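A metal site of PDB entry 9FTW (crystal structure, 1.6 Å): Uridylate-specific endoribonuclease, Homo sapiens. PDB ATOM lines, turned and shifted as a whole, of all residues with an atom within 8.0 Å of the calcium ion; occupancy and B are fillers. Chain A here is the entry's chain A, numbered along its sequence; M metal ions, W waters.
The backbone carbonyl oxygen (O) of Val 331 is in hydrogen-bond range of the backbone NH (N) of Gly 323, at 2.8 Å.
Within 4 Å of the calcium ion: Asp 322, Gly 323, Trp 325 and Asp 330.
The nearest printed residue that does not touch the calcium ion is Pro 324 (4.3 Å).
OD1 of Asp 322 binds the calcium ion.
O of Gly 323 is bound to the calcium ion (2.3 Å).
The calcium ion is bound by O of Trp 325 (2.4 Å).
Water W2 binds the calcium ion (2.4 Å).
OD2 of Asp 330 binds the calcium ion (2.4 Å).
The calcium ion is bound by water W1 (2.4 Å).
The calcium ion is bound by the side-chain carboxylate (OD1) of Asp 330, at 2.6 Å.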
ATOM      1  N   LEU A 163     -20.808   8.394  32.030  1.00  0.00           N
ATOM      2  CA  LEU A 163     -22.203   8.690  31.706  1.00  0.00           C
ATOM      3  C   LEU A 163     -23.070   7.473  31.928  1.00  0.00           C
ATOM      4  O   LEU A 163     -22.636   6.349  31.673  1.00  0.00           O
ATOM      5  CB  LEU A 163     -22.344   9.054  30.216  1.00  0.00           C
ATOM      6  CG  LEU A 163     -22.020  10.469  29.737  1.00  0.00           C
ATOM      7  CD1 LEU A 163     -22.361  10.575  28.196  1.00  0.00           C
ATOM      8  CD2 LEU A 163     -22.798  11.539  30.563  1.00  0.00           C
ATOM      9  N   TYR A 321     -31.837  10.320  21.695  1.00  0.00           N
ATOM     10  CA  TYR A 321     -30.749  10.244  20.748  1.00  0.00           C
ATOM     11  C   TYR A 321     -29.417  10.278  21.477  1.00  0.00           C
ATOM     12  O   TYR A 321     -29.205  11.052  22.431  1.00  0.00           O
ATOM     13  CB  TYR A 321     -30.883  11.426  19.756  1.00  0.00           C
ATOM     14  CG  TYR A 321     -29.679  11.665  18.876  1.00  0.00           C
ATOM     15  CD1 TYR A 321     -29.501  10.947  17.707  1.00  0.00           C
ATOM     16  CD2 TYR A 321     -28.737  12.634  19.200  1.00  0.00           C
ATOM     17  CE1 TYR A 321     -28.380  11.138  16.918  1.00  0.00           C
ATOM     18  CE2 TYR A 321     -27.628  12.843  18.391  1.00  0.00           C
ATOM     19  CZ  TYR A 321     -27.487  12.141  17.219  1.00  0.00           C
ATOM     20  OH  TYR A 321     -26.382  12.341  16.410  1.00  0.00           O
ATOM     21  N   ASP A 322     -28.494   9.454  20.978  1.00  0.00           N
ATOM     22  CA  ASP A 322     -27.135   9.368  21.462  1.00  0.00           C
ATOM     23  C   ASP A 322     -26.303   9.359  20.175  1.00  0.00           C
ATOM     24  O   ASP A 322     -26.466   8.443  19.348  1.00  0.00           O
ATOM     25  CB  ASP A 322     -26.946   8.060  22.241  1.00  0.00           C
ATOM     26  CG  ASP A 322     -25.576   7.869  22.850  1.00  0.00           C
ATOM     27  OD1 ASP A 322     -24.579   8.453  22.324  1.00  0.00           O
ATOM     28  OD2 ASP A 322     -25.471   7.086  23.822  1.00  0.00           O
ATOM     29  N   GLY A 323     -25.513  10.409  19.988  1.00  0.00           N
ATOM     30  CA  GLY A 323     -24.734  10.636  18.780  1.00  0.00           C
ATOM     31  C   GLY A 323     -23.754   9.543  18.433  1.00  0.00           C
ATOM     32  O   GLY A 323     -23.345   8.787  19.311  1.00  0.00           O
ATOM     33  N   PRO A 324     -23.303   9.493  17.152  1.00  0.00           N
ATOM     34  CA  PRO A 324     -22.411   8.390  16.736  1.00  0.00           C
ATOM     35  C   PRO A 324     -21.034   8.391  17.376  1.00  0.00           C
ATOM     36  O   PRO A 324     -20.355   7.380  17.339  1.00  0.00           O
ATOM     37  CB  PRO A 324     -22.290   8.576  15.209  1.00  0.00           C
ATOM     38  CG  PRO A 324     -22.634  10.002  14.965  1.00  0.00           C
ATOM     39  CD  PRO A 324     -23.699  10.313  15.996  1.00  0.00           C
ATOM     40  N   TRP A 325     -20.608   9.520  17.966  1.00  0.00           N
ATOM     41  CA  TRP A 325     -19.304   9.583  18.644  1.00  0.00           C
ATOM     42  C   TRP A 325     -19.277   8.576  19.797  1.00  0.00           C
ATOM     43  O   TRP A 325     -20.291   8.443  20.518  1.00  0.00           O
ATOM     44  CB  TRP A 325     -19.095  11.030  19.202  1.00  0.00           C
ATOM     45  CG  TRP A 325     -19.169  12.093  18.148  1.00  0.00           C
ATOM     46  CD1 TRP A 325     -18.152  12.538  17.354  1.00  0.00           C
ATOM     47  CD2 TRP A 325     -20.353  12.768  17.701  1.00  0.00           C
ATOM     48  NE1 TRP A 325     -18.622  13.446  16.438  1.00  0.00           N
ATOM     49  CE2 TRP A 325     -19.962  13.646  16.656  1.00  0.00           C
ATOM     50  CE3 TRP A 325     -21.699  12.757  18.098  1.00  0.00           C
ATOM     51  CZ2 TRP A 325     -20.898  14.370  15.912  1.00  0.00           C
ATOM     52  CZ3 TRP A 325     -22.601  13.539  17.400  1.00  0.00           C
ATOM     53  CH2 TRP A 325     -22.205  14.299  16.299  1.00  0.00           C
ATOM     54  N   ASP A 326     -18.182   7.804  19.930  1.00  0.00           N
ATOM     55  CA  ASP A 326     -17.970   6.862  21.042  1.00  0.00           C
ATOM     56  C   ASP A 326     -16.831   7.417  21.934  1.00  0.00           C
ATOM     57  O   ASP A 326     -15.995   6.682  22.438  1.00  0.00           O
ATOM     58  CB  ASP A 326     -17.587   5.460  20.477  1.00  0.00           C
ATOM     59  CG  ASP A 326     -17.640   4.357  21.508  1.00  0.00           C
ATOM     60  OD1 ASP A 326     -18.365   4.519  22.530  1.00  0.00           O
ATOM     61  OD2 ASP A 326     -16.950   3.324  21.310  1.00  0.00           O
ATOM     62  N   SER A 327     -16.788   8.734  22.089  1.00  0.00           N
ATOM     63  CA  SER A 327     -15.750   9.436  22.828  1.00  0.00           C
ATOM     64  C   SER A 327     -16.265  10.869  23.093  1.00  0.00           C
ATOM     65  O   SER A 327     -17.311  11.229  22.541  1.00  0.00           O
ATOM     66  CB  SER A 327     -14.463   9.524  21.988  1.00  0.00           C
ATOM     67  OG  SER A 327     -14.662  10.291  20.817  1.00  0.00           O
ATOM     68  N   PRO A 329     -15.999  14.862  22.538  1.00  0.00           N
ATOM     69  CA  PRO A 329     -17.403  15.242  22.790  1.00  0.00           C
ATOM     70  C   PRO A 329     -18.418  14.288  22.170  1.00  0.00           C
ATOM     71  O   PRO A 329     -18.232  13.816  21.034  1.00  0.00           O
ATOM     72  CB  PRO A 329     -17.492  16.645  22.155  1.00  0.00           C
ATOM     73  CG  PRO A 329     -16.534  16.539  20.965  1.00  0.00           C
ATOM     74  CD  PRO A 329     -15.368  15.741  21.524  1.00  0.00           C
ATOM     75  N   ASP A 330     -19.472  13.974  22.907  1.00  0.00           N
ATOM     76  CA  ASP A 330     -20.574  13.182  22.388  1.00  0.00           C
ATOM     77  C   ASP A 330     -21.819  14.098  22.352  1.00  0.00           C
ATOM     78  O   ASP A 330     -21.719  15.280  22.746  1.00  0.00           O
ATOM     79  CB  ASP A 330     -20.805  11.930  23.266  1.00  0.00           C
ATOM     80  CG  ASP A 330     -21.510  10.757  22.589  1.00  0.00           C
ATOM     81  OD1 ASP A 330     -22.085  10.938  21.475  1.00  0.00           O
ATOM     82  OD2 ASP A 330     -21.563   9.670  23.210  1.00  0.00           O
ATOM     83  N   VAL A 331     -22.973  13.612  21.865  1.00  0.00           N
ATOM     84  CA  VAL A 331     -24.193  14.439  21.846  1.00  0.00           C
ATOM     85  C   VAL A 331     -25.306  13.574  22.408  1.00  0.00           C
ATOM     86  O   VAL A 331     -25.433  12.405  22.012  1.00  0.00           O
ATOM     87  CB  VAL A 331     -24.534  14.952  20.417  1.00  0.00           C
ATOM     88  CG1 VAL A 331     -25.930  15.575  20.362  1.00  0.00           C
ATOM     89  CG2 VAL A 331     -23.477  15.945  19.928  1.00  0.00           C
ATOM     90  N   LEU A 332     -26.067  14.111  23.347  1.00  0.00           N
ATOM     91  CA  LEU A 332     -27.276  13.422  23.890  1.00  0.00           C
ATOM     92  C   LEU A 332     -28.459  14.364  23.750  1.00  0.00           C
ATOM     93  O   LEU A 332     -28.297  15.549  24.059  1.00  0.00           O
ATOM     94  CB  LEU A 332     -27.119  13.117  25.374  1.00  0.00           C
ATOM     95  CG  LEU A 332     -26.513  11.787  25.817  1.00  0.00           C
ATOM     96  CD1 LEU A 332     -26.407  11.766  27.332  1.00  0.00           C
ATOM     97  CD2 LEU A 332     -27.375  10.564  25.365  1.00  0.00           C
HETATM   98 CA    CA M   1     -22.477   8.364  21.403  1.00  0.00          CA
HETATM   99  O   HOH W   1     -21.626   6.792  23.059  1.00  0.00           O
HETATM  100  O   HOH W   2     -22.885   6.181  20.496  1.00  0.00           O
